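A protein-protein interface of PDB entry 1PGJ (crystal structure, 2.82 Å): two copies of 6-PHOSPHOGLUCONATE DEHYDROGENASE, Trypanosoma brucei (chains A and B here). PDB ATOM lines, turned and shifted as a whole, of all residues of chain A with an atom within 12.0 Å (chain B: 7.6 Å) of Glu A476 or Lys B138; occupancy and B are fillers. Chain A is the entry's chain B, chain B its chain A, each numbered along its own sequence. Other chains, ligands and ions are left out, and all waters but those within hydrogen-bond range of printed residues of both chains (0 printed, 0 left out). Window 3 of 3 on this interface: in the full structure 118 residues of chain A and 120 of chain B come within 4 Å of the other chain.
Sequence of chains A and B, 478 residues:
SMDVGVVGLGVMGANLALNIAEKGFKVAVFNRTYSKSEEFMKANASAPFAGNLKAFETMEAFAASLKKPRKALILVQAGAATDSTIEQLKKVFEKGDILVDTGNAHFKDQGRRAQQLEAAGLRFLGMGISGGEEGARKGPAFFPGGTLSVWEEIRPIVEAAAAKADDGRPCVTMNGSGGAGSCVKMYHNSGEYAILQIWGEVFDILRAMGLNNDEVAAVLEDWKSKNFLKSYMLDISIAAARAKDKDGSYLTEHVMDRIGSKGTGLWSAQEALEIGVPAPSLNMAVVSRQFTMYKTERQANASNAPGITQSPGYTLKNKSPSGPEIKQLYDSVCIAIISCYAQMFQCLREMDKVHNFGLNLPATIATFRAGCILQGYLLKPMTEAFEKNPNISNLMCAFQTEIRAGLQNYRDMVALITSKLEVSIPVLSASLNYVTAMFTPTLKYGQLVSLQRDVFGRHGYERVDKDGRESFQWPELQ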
ATOM      1  N   ASP A 454     -37.021  25.009  -6.714  1.00  0.00           N
ATOM      2  CA  ASP A 454     -37.176  23.675  -7.281  1.00  0.00           C
ATOM      3  C   ASP A 454     -36.369  23.536  -8.587  1.00  0.00           C
ATOM      4  O   ASP A 454     -35.591  22.594  -8.766  1.00  0.00           O
ATOM      5  CB  ASP A 454     -38.641  23.353  -7.561  1.00  0.00           C
ATOM      6  CG  ASP A 454     -38.848  21.885  -7.871  1.00  0.00           C
ATOM      7  OD1 ASP A 454     -38.533  21.066  -6.989  1.00  0.00           O
ATOM      8  OD2 ASP A 454     -39.285  21.542  -8.989  1.00  0.00           O
ATOM      9  N   VAL A 455     -36.508  24.518  -9.463  1.00  0.00           N
ATOM     10  CA  VAL A 455     -35.830  24.514 -10.738  1.00  0.00           C
ATOM     11  C   VAL A 455     -34.389  24.077 -10.663  1.00  0.00           C
ATOM     12  O   VAL A 455     -34.008  23.080 -11.261  1.00  0.00           O
ATOM     13  CB  VAL A 455     -35.888  25.899 -11.386  1.00  0.00           C
ATOM     14  CG1 VAL A 455     -35.231  25.877 -12.752  1.00  0.00           C
ATOM     15  CG2 VAL A 455     -37.343  26.371 -11.483  1.00  0.00           C
ATOM     16  N   PHE A 456     -33.588  24.785  -9.888  1.00  0.00           N
ATOM     17  CA  PHE A 456     -32.169  24.455  -9.817  1.00  0.00           C
ATOM     18  C   PHE A 456     -31.703  23.484  -8.730  1.00  0.00           C
ATOM     19  O   PHE A 456     -30.761  22.694  -8.936  1.00  0.00           O
ATOM     20  CB  PHE A 456     -31.356  25.748  -9.724  1.00  0.00           C
ATOM     21  CG  PHE A 456     -31.649  26.592  -8.490  1.00  0.00           C
ATOM     22  CD1 PHE A 456     -31.099  26.258  -7.246  1.00  0.00           C
ATOM     23  CD2 PHE A 456     -32.409  27.765  -8.591  1.00  0.00           C
ATOM     24  CE1 PHE A 456     -31.293  27.075  -6.136  1.00  0.00           C
ATOM     25  CE2 PHE A 456     -32.603  28.588  -7.479  1.00  0.00           C
ATOM     26  CZ  PHE A 456     -32.045  28.243  -6.254  1.00  0.00           C
ATOM     27  N   ARG A 458     -33.814  21.387  -7.013  1.00  0.00           N
ATOM     28  CA  ARG A 458     -34.736  20.242  -6.895  1.00  0.00           C
ATOM     29  C   ARG A 458     -35.217  20.049  -5.437  1.00  0.00           C
ATOM     30  O   ARG A 458     -35.424  18.926  -4.991  1.00  0.00           O
ATOM     31  CB  ARG A 458     -34.082  18.934  -7.400  1.00  0.00           C
ATOM     32  CG  ARG A 458     -33.291  18.984  -8.733  1.00  0.00           C
ATOM     33  CD  ARG A 458     -33.924  19.832  -9.874  1.00  0.00           C
ATOM     34  NE  ARG A 458     -35.375  19.716  -9.988  1.00  0.00           N
ATOM     35  CZ  ARG A 458     -36.014  18.605 -10.318  1.00  0.00           C
ATOM     36  NH1 ARG A 458     -35.329  17.491 -10.583  1.00  0.00           N
ATOM     37  NH2 ARG A 458     -37.340  18.596 -10.336  1.00  0.00           N
ATOM     38  N   PHE A 472     -41.651  19.644  -9.622  1.00  0.00           N
ATOM     39  CA  PHE A 472     -41.999  19.682 -11.039  1.00  0.00           C
ATOM     40  C   PHE A 472     -40.850  19.166 -11.940  1.00  0.00           C
ATOM     41  O   PHE A 472     -39.774  18.836 -11.448  1.00  0.00           O
ATOM     42  CB  PHE A 472     -42.365  21.123 -11.407  1.00  0.00           C
ATOM     43  CG  PHE A 472     -43.279  21.240 -12.590  1.00  0.00           C
ATOM     44  CD1 PHE A 472     -44.448  20.501 -12.658  1.00  0.00           C
ATOM     45  CD2 PHE A 472     -42.993  22.129 -13.621  1.00  0.00           C
ATOM     46  CE1 PHE A 472     -45.319  20.651 -13.733  1.00  0.00           C
ATOM     47  CE2 PHE A 472     -43.871  22.284 -14.704  1.00  0.00           C
ATOM     48  CZ  PHE A 472     -45.032  21.542 -14.752  1.00  0.00           C
ATOM     49  N   GLN A 473     -41.113  19.017 -13.239  1.00  0.00           N
ATOM     50  CA  GLN A 473     -40.095  18.591 -14.206  1.00  0.00           C
ATOM     51  C   GLN A 473     -39.834  19.808 -15.076  1.00  0.00           C
ATOM     52  O   GLN A 473     -40.775  20.372 -15.646  1.00  0.00           O
ATOM     53  CB  GLN A 473     -40.600  17.443 -15.065  1.00  0.00           C
ATOM     54  CG  GLN A 473     -40.663  16.120 -14.326  1.00  0.00           C
ATOM     55  CD  GLN A 473     -39.291  15.590 -13.951  1.00  0.00           C
ATOM     56  OE1 GLN A 473     -38.418  15.424 -14.811  1.00  0.00           O
ATOM     57  NE2 GLN A 473     -39.095  15.320 -12.664  1.00  0.00           N
ATOM     58  N   TRP A 474     -38.572  20.212 -15.187  1.00  0.00           N
ATOM     59  CA  TRP A 474     -38.251  21.414 -15.946  1.00  0.00           C
ATOM     60  C   TRP A 474     -37.386  21.236 -17.185  1.00  0.00           C
ATOM     61  O   TRP A 474     -36.585  20.295 -17.288  1.00  0.00           O
ATOM     62  CB  TRP A 474     -37.551  22.436 -15.037  1.00  0.00           C
ATOM     63  CG  TRP A 474     -38.190  22.656 -13.700  1.00  0.00           C
ATOM     64  CD1 TRP A 474     -37.839  22.059 -12.518  1.00  0.00           C
ATOM     65  CD2 TRP A 474     -39.266  23.556 -13.392  1.00  0.00           C
ATOM     66  NE1 TRP A 474     -38.620  22.537 -11.500  1.00  0.00           N
ATOM     67  CE2 TRP A 474     -39.503  23.454 -12.002  1.00  0.00           C
ATOM     68  CE3 TRP A 474     -40.044  24.436 -14.156  1.00  0.00           C
ATOM     69  CZ2 TRP A 474     -40.501  24.210 -11.352  1.00  0.00           C
ATOM     70  CZ3 TRP A 474     -41.035  25.190 -13.505  1.00  0.00           C
ATOM     71  CH2 TRP A 474     -41.251  25.066 -12.117  1.00  0.00           C
ATOM     72  N   PRO A 475     -37.529  22.159 -18.143  1.00  0.00           N
ATOM     73  CA  PRO A 475     -36.760  22.139 -19.385  1.00  0.00           C
ATOM     74  C   PRO A 475     -35.298  22.410 -19.037  1.00  0.00           C
ATOM     75  O   PRO A 475     -35.003  23.003 -17.981  1.00  0.00           O
ATOM     76  CB  PRO A 475     -37.326  23.333 -20.151  1.00  0.00           C
ATOM     77  CG  PRO A 475     -38.734  23.457 -19.629  1.00  0.00           C
ATOM     78  CD  PRO A 475     -38.535  23.238 -18.166  1.00  0.00           C
ATOM     79  N   GLU A 476     -34.380  21.944 -19.883  1.00  0.00           N
ATOM     80  CA  GLU A 476     -32.969  22.206 -19.641  1.00  0.00           C
ATOM     81  C   GLU A 476     -32.882  23.698 -19.888  1.00  0.00           C
ATOM     82  O   GLU A 476     -33.687  24.242 -20.667  1.00  0.00           O
ATOM     83  CB  GLU A 476     -32.072  21.469 -20.636  1.00  0.00           C
ATOM     84  CG  GLU A 476     -31.887  19.977 -20.372  1.00  0.00           C
ATOM     85  CD  GLU A 476     -31.098  19.275 -21.481  1.00  0.00           C
ATOM     86  OE1 GLU A 476     -31.625  19.172 -22.622  1.00  0.00           O
ATOM     87  OE2 GLU A 476     -29.953  18.830 -21.215  1.00  0.00           O
ATOM     88  N   LEU A 477     -31.976  24.368 -19.179  1.00  0.00           N
ATOM     89  CA  LEU A 477     -31.822  25.802 -19.344  1.00  0.00           C
ATOM     90  C   LEU A 477     -30.452  26.229 -19.842  1.00  0.00           C
ATOM     91  O   LEU A 477     -30.315  27.341 -20.322  1.00  0.00           O
ATOM     92  CB  LEU A 477     -32.188  26.549 -18.058  1.00  0.00           C
ATOM     93  CG  LEU A 477     -33.669  26.509 -17.637  1.00  0.00           C
ATOM     94  CD1 LEU A 477     -33.821  27.150 -16.271  1.00  0.00           C
ATOM     95  CD2 LEU A 477     -34.556  27.216 -18.662  1.00  0.00           C
ATOM     96  N   GLN A 478     -29.476  25.325 -19.801  1.00  0.00           N
ATOM     97  CA  GLN A 478     -28.108  25.619 -20.235  1.00  0.00           C
ATOM     98  C   GLN A 478     -27.610  24.770 -21.418  1.00  0.00           C
ATOM     99  O   GLN A 478     -26.441  24.309 -21.394  1.00  0.00           O
ATOM    100  CB  GLN A 478     -27.154  25.469 -19.046  1.00  0.00           C
ATOM    101  CG  GLN A 478     -27.128  26.650 -18.097  1.00  0.00           C
ATOM    102  CD  GLN A 478     -26.485  26.334 -16.754  1.00  0.00           C
ATOM    103  OE1 GLN A 478     -26.826  26.937 -15.746  1.00  0.00           O
ATOM    104  NE2 GLN A 478     -25.534  25.389 -16.738  1.00  0.00           N
ATOM    105  OXT GLN A 478     -28.392  24.581 -22.379  1.00  0.00           O
ATOM    106  N   ASN B  15     -23.994  13.716 -10.292  1.00  0.00           N
ATOM    107  CA  ASN B  15     -23.849  14.452 -11.537  1.00  0.00           C
ATOM    108  C   ASN B  15     -22.402  14.861 -11.706  1.00  0.00           C
ATOM    109  O   ASN B  15     -21.827  14.718 -12.794  1.00  0.00           O
ATOM    110  CB  ASN B  15     -24.720  15.709 -11.538  1.00  0.00           C
ATOM    111  CG  ASN B  15     -26.196  15.427 -11.855  1.00  0.00           C
ATOM    112  OD1 ASN B  15     -26.556  14.964 -12.945  1.00  0.00           O
ATOM    113  ND2 ASN B  15     -27.065  15.772 -10.908  1.00  0.00           N
ATOM    114  N   LEU B  16     -21.818  15.390 -10.632  1.00  0.00           N
ATOM    115  CA  LEU B  16     -20.427  15.818 -10.666  1.00  0.00           C
ATOM    116  C   LEU B  16     -19.573  14.644 -11.103  1.00  0.00           C
ATOM    117  O   LEU B  16     -18.871  14.730 -12.093  1.00  0.00           O
ATOM    118  CB  LEU B  16     -19.950  16.321  -9.307  1.00  0.00           C
ATOM    119  CG  LEU B  16     -18.472  16.714  -9.328  1.00  0.00           C
ATOM    120  CD1 LEU B  16     -18.283  17.897 -10.232  1.00  0.00           C
ATOM    121  CD2 LEU B  16     -17.963  17.023  -7.959  1.00  0.00           C
ATOM    122  N   ASN B  19     -19.782  14.007 -14.801  1.00  0.00           N
ATOM    123  CA  ASN B  19     -19.078  15.113 -15.438  1.00  0.00           C
ATOM    124  C   ASN B  19     -17.567  14.785 -15.502  1.00  0.00           C
ATOM    125  O   ASN B  19     -16.968  14.679 -16.588  1.00  0.00           O
ATOM    126  CB  ASN B  19     -19.353  16.373 -14.596  1.00  0.00           C
ATOM    127  CG  ASN B  19     -18.647  17.629 -15.105  1.00  0.00           C
ATOM    128  OD1 ASN B  19     -17.653  17.557 -15.806  1.00  0.00           O
ATOM    129  ND2 ASN B  19     -19.140  18.790 -14.689  1.00  0.00           N
ATOM    130  N   GLU B  22     -16.844  11.661 -17.670  1.00  0.00           N
ATOM    131  CA  GLU B  22     -16.953  11.990 -19.078  1.00  0.00           C
ATOM    132  C   GLU B  22     -15.780  12.795 -19.565  1.00  0.00           C
ATOM    133  O   GLU B  22     -15.523  12.849 -20.770  1.00  0.00           O
ATOM    134  CB  GLU B  22     -18.233  12.757 -19.321  1.00  0.00           C
ATOM    135  CG  GLU B  22     -18.525  12.946 -20.751  1.00  0.00           C
ATOM    136  CD  GLU B  22     -19.589  13.972 -20.955  1.00  0.00           C
ATOM    137  OE1 GLU B  22     -19.287  15.185 -20.741  1.00  0.00           O
ATOM    138  OE2 GLU B  22     -20.715  13.563 -21.328  1.00  0.00           O
ATOM    139  N   LYS B  23     -15.131  13.490 -18.634  1.00  0.00           N
ATOM    140  CA  LYS B  23     -13.957  14.295 -18.959  1.00  0.00           C
ATOM    141  C   LYS B  23     -12.756  13.349 -19.089  1.00  0.00           C
ATOM    142  O   LYS B  23     -11.638  13.765 -19.410  1.00  0.00           O
ATOM    143  CB  LYS B  23     -13.719  15.382 -17.895  1.00  0.00           C
ATOM    144  CG  LYS B  23     -14.894  16.358 -17.710  1.00  0.00           C
ATOM    145  CD  LYS B  23     -15.201  17.159 -18.973  1.00  0.00           C
ATOM    146  CE  LYS B  23     -16.202  18.285 -18.729  1.00  0.00           C
ATOM    147  NZ  LYS B  23     -17.571  17.925 -19.187  1.00  0.00           N
ATOM    148  N   GLY B 132     -26.169  23.893  -9.385  1.00  0.00           N
ATOM    149  CA  GLY B 132     -27.347  23.058  -9.223  1.00  0.00           C
ATOM    150  C   GLY B 132     -27.147  21.710  -9.903  1.00  0.00           C
ATOM    151  O   GLY B 132     -26.027  21.314 -10.230  1.00  0.00           O
ATOM    152  N   GLU B 133     -28.242  21.012 -10.154  1.00  0.00           N
ATOM    153  CA  GLU B 133     -28.196  19.695 -10.792  1.00  0.00           C
ATOM    154  C   GLU B 133     -27.558  19.740 -12.182  1.00  0.00           C
ATOM    155  O   GLU B 133     -26.614  19.004 -12.466  1.00  0.00           O
ATOM    156  CB  GLU B 133     -29.614  19.140 -10.872  1.00  0.00           C
ATOM    157  CG  GLU B 133     -29.777  17.811 -11.557  1.00  0.00           C
ATOM    158  CD  GLU B 133     -31.240  17.510 -11.775  1.00  0.00           C
ATOM    159  OE1 GLU B 133     -31.855  18.168 -12.654  1.00  0.00           O
ATOM    160  OE2 GLU B 133     -31.784  16.650 -11.043  1.00  0.00           O
ATOM    161  N   GLU B 134     -28.081  20.606 -13.040  1.00  0.00           N
ATOM    162  CA  GLU B 134     -27.570  20.770 -14.392  1.00  0.00           C
ATOM    163  C   GLU B 134     -26.116  21.265 -14.374  1.00  0.00           C
ATOM    164  O   GLU B 134     -25.258  20.760 -15.104  1.00  0.00           O
ATOM    165  CB  GLU B 134     -28.415  21.795 -15.130  1.00  0.00           C
ATOM    166  CG  GLU B 134     -29.399  21.231 -16.123  1.00  0.00           C
ATOM    167  CD  GLU B 134     -29.993  22.322 -16.999  1.00  0.00           C
ATOM    168  OE1 GLU B 134     -31.032  22.909 -16.597  1.00  0.00           O
ATOM    169  OE2 GLU B 134     -29.409  22.608 -18.076  1.00  0.00           O
ATOM    170  N   GLY B 135     -25.849  22.279 -13.561  1.00  0.00           N
ATOM    171  CA  GLY B 135     -24.506  22.819 -13.478  1.00  0.00           C
ATOM    172  C   GLY B 135     -23.484  21.767 -13.108  1.00  0.00           C
ATOM    173  O   GLY B 135     -22.399  21.753 -13.674  1.00  0.00           O
ATOM    174  N   ALA B 136     -23.837  20.891 -12.166  1.00  0.00           N
ATOM    175  CA  ALA B 136     -22.957  19.815 -11.694  1.00  0.00           C
ATOM    176  C   ALA B 136     -22.588  18.883 -12.826  1.00  0.00           C
ATOM    177  O   ALA B 136     -21.425  18.525 -12.991  1.00  0.00           O
ATOM    178  CB  ALA B 136     -23.639  19.023 -10.587  1.00  0.00           C
ATOM    179  N   ARG B 137     -23.595  18.487 -13.594  1.00  0.00           N
ATOM    180  CA  ARG B 137     -23.412  17.605 -14.733  1.00  0.00           C
ATOM    181  C   ARG B 137     -22.684  18.254 -15.924  1.00  0.00           C
ATOM    182  O   ARG B 137     -21.837  17.617 -16.565  1.00  0.00           O
ATOM    183  CB  ARG B 137     -24.767  17.104 -15.203  1.00  0.00           C
ATOM    184  CG  ARG B 137     -24.683  16.203 -16.392  1.00  0.00           C
ATOM    185  CD  ARG B 137     -23.834  14.993 -16.068  1.00  0.00           C
ATOM    186  NE  ARG B 137     -23.723  14.126 -17.233  1.00  0.00           N
ATOM    187  CZ  ARG B 137     -22.777  14.236 -18.166  1.00  0.00           C
ATOM    188  NH1 ARG B 137     -21.835  15.172 -18.070  1.00  0.00           N
ATOM    189  NH2 ARG B 137     -22.814  13.445 -19.233  1.00  0.00           N
ATOM    190  N   LYS B 138     -22.982  19.519 -16.201  1.00  0.00           N
ATOM    191  CA  LYS B 138     -22.388  20.192 -17.345  1.00  0.00           C
ATOM    192  C   LYS B 138     -21.151  21.047 -17.114  1.00  0.00           C
ATOM    193  O   LYS B 138     -20.281  21.184 -18.007  1.00  0.00           O
ATOM    194  CB  LYS B 138     -23.454  21.005 -18.055  1.00  0.00           C
ATOM    195  CG  LYS B 138     -24.669  20.210 -18.464  1.00  0.00           C
ATOM    196  CD  LYS B 138     -25.594  21.109 -19.228  1.00  0.00           C
ATOM    197  CE  LYS B 138     -26.933  20.447 -19.477  1.00  0.00           C
ATOM    198  NZ  LYS B 138     -27.868  21.378 -20.188  1.00  0.00           N
ATOM    199  N   GLY B 139     -21.085  21.675 -15.951  1.00  0.00           N
ATOM    200  CA  GLY B 139     -19.937  22.522 -15.655  1.00  0.00           C
ATOM    201  C   GLY B 139     -20.294  23.667 -14.732  1.00  0.00           C
ATOM    202  O   GLY B 139     -20.845  24.696 -15.168  1.00  0.00           O
ATOM    203  N   PRO B 140     -20.003  23.501 -13.439  1.00  0.00           N
ATOM    204  CA  PRO B 140     -20.285  24.494 -12.415  1.00  0.00           C
ATOM    205  C   PRO B 140     -19.111  25.400 -12.207  1.00  0.00           C
ATOM    206  O   PRO B 140     -18.132  25.366 -12.966  1.00  0.00           O
ATOM    207  CB  PRO B 140     -20.485  23.620 -11.183  1.00  0.00           C
ATOM    208  CG  PRO B 140     -19.444  22.565 -11.377  1.00  0.00           C
ATOM    209  CD  PRO B 140     -19.532  22.243 -12.827  1.00  0.00           C
ATOM    210  N   ALA B 160     -11.033  21.206 -15.539  1.00  0.00           N
ATOM    211  CA  ALA B 160     -11.635  20.447 -16.617  1.00  0.00           C
ATOM    212  C   ALA B 160     -13.145  20.320 -16.509  1.00  0.00           C
ATOM    213  O   ALA B 160     -13.842  20.268 -17.517  1.00  0.00           O
ATOM    214  CB  ALA B 160     -11.013  19.076 -16.666  1.00  0.00           C
ATOM    215  N   ALA B 161     -13.643  20.221 -15.281  1.00  0.00           N
ATOM    216  CA  ALA B 161     -15.079  20.067 -15.034  1.00  0.00           C
ATOM    217  C   ALA B 161     -15.795  21.381 -14.824  1.00  0.00           C
ATOM    218  O   ALA B 161     -17.025  21.427 -14.758  1.00  0.00           O
ATOM    219  CB  ALA B 161     -15.312  19.167 -13.836  1.00  0.00           C
ATOM    220  N   ALA B 162     -15.029  22.450 -14.673  1.00  0.00           N
ATOM    221  CA  ALA B 162     -15.627  23.758 -14.466  1.00  0.00           C
ATOM    222  C   ALA B 162     -16.305  24.214 -15.746  1.00  0.00           C
ATOM    223  O   ALA B 162     -16.045  23.667 -16.821  1.00  0.00           O
ATOM    224  CB  ALA B 162     -14.566  24.756 -14.088  1.00  0.00           C
ATOM    225  N   ALA B 163     -17.205  25.178 -15.608  1.00  0.00           N
ATOM    226  CA  ALA B 163     -17.871  25.772 -16.739  1.00  0.00           C
ATOM    227  C   ALA B 163     -16.810  26.717 -17.307  1.00  0.00           C
ATOM    228  O   ALA B 163     -15.921  27.168 -16.567  1.00  0.00           O
ATOM    229  CB  ALA B 163     -19.061  26.564 -16.267  1.00  0.00           C
ATOM    230  N   LYS B 164     -16.863  26.979 -18.612  1.00  0.00           N
ATOM    231  CA  LYS B 164     -15.914  27.880 -19.281  1.00  0.00           C
ATOM    232  C   LYS B 164     -16.687  29.165 -19.592  1.00  0.00           C
ATOM    233  O   LYS B 164     -17.800  29.097 -20.107  1.00  0.00           O
ATOM    234  CB  LYS B 164     -15.466  27.268 -20.622  1.00  0.00           C
ATOM    235  CG  LYS B 164     -14.025  26.778 -20.759  1.00  0.00           C
ATOM    236  CD  LYS B 164     -13.847  25.315 -20.398  1.00  0.00           C
ATOM    237  CE  LYS B 164     -13.797  25.096 -18.855  1.00  0.00           C
ATOM    238  NZ  LYS B 164     -13.478  23.675 -18.422  1.00  0.00           N
ATOM    239  N   TYR B 232     -29.432  33.635 -15.569  1.00  0.00           N
ATOM    240  CA  TYR B 232     -29.999  32.328 -15.290  1.00  0.00           C
ATOM    241  C   TYR B 232     -31.267  32.496 -14.461  1.00  0.00           C
ATOM    242  O   TYR B 232     -32.311  31.940 -14.791  1.00  0.00           O
ATOM    243  CB  TYR B 232     -28.993  31.490 -14.509  1.00  0.00           C
ATOM    244  CG  TYR B 232     -29.490  30.111 -14.154  1.00  0.00           C
ATOM    245  CD1 TYR B 232     -29.520  29.093 -15.108  1.00  0.00           C
ATOM    246  CD2 TYR B 232     -29.880  29.807 -12.850  1.00  0.00           C
ATOM    247  CE1 TYR B 232     -29.913  27.799 -14.773  1.00  0.00           C
ATOM    248  CE2 TYR B 232     -30.281  28.502 -12.497  1.00  0.00           C
ATOM    249  CZ  TYR B 232     -30.280  27.502 -13.462  1.00  0.00           C
ATOM    250  OH  TYR B 232     -30.513  26.198 -13.096  1.00  0.00           O
ATOM    251  N   GLY B 371     -21.854  28.723 -15.054  1.00  0.00           N
ATOM    252  CA  GLY B 371     -22.031  27.645 -14.099  1.00  0.00           C
ATOM    253  C   GLY B 371     -22.789  27.978 -12.831  1.00  0.00           C
ATOM    254  O   GLY B 371     -23.778  27.298 -12.499  1.00  0.00           O
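Among the printed residues, merely in contact across the chains: Gln A478 with Tyr B232, Phe A456 with Gly B132, Phe A456 with Tyr B232 and Glu A476 with Glu B134.
N of Glu B133 sits at hydrogen-bond distance from O of Phe A456 (3.3 Å). The guanidinium group of Arg A458 lies within salt-bridge range of the side-chain carboxylate of Glu B133 (3.7 Å). The side-chain carboxylate (OE1) of Glu B134 is in hydrogen-bond range of the backbone NH (N) of Leu A477 (3.1 Å). N of Gln A478 sits at hydrogen-bond distance from OE2 of Glu B134 (3.2 Å). NZ of Lys B138 lies within salt-bridge range of OE2 of Glu A476 (3.4 Å). The side-chain amino group (NZ) of Lys B138 is in salt-bridge range of the chain-end carboxylate (O) of Gln A478 (3.5 Å).
The side-chain carboxylate (OE2) of Glu B134 is in salt-bridge range of the side-chain amino group (NZ) of Lys B138 (2.9 Å). The guanidinium group (NH2) of Arg A458 lies within salt-bridge range of the side-chain carboxylate (OD2) of Asp A454, 3.8 Å away. The guanidinium group of Arg A458 is in hydrogen-bond range of the backbone carbonyl oxygen of Phe A472 (2.7 Å).
No position is printed for both chains. Of the 10 pairs that touch across the chains among the printed residues, none has its exchanged pair printed and touching as well.
Of the 11 printed residues of chain A, 5 touch a printed residue of chain B. Hydrophobic or aromatic side chains of chain A within 4 Å of the printed part of chain B: Phe A456. Of the 21 printed residues of chain B, 5 touch a printed residue of chain A. Hydrophobic or aromatic side chains of chain B that line the printed part of chain A: Tyr B232.
Of chain B, only Glu B134 and Lys B138 come within 4 Å of Glu A476. Lys B138 touches just these residues of chain A: Glu A476 (3.4 Å) and Gln A478 (3.5 Å). Asn B19 touches none of the printed residues of chain A. Glu B134 touches three residues of chain A. Gly B135 touches none of the printed residues of chain A. No residue of chain A comes within 4 Å of Ala B136. No residue of chain A comes within 4 Å of Gly B139. No residue of chain A comes within 4 Å of Pro B140. No residue of chain A comes within 4 Å of Ala B161. Of the printed residues of chain A, Tyr B232 touches Phe A456 and Gln A478. Printed residues of chain A within 4 Å of Gly B132: Phe A456 (3.4 Å). Of the printed residues of chain B, Leu A477 touches Glu B134 (3.1 Å). The nearest residue of chain B that does not touch Glu A476 is Tyr B232 (7.2 Å). The nearest residue of chain A that does not touch Lys B138 is Leu A477 (5.2 Å). The nearest printed residue of chain B that does not touch Arg A458 is Glu B134 (6.7 Å).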
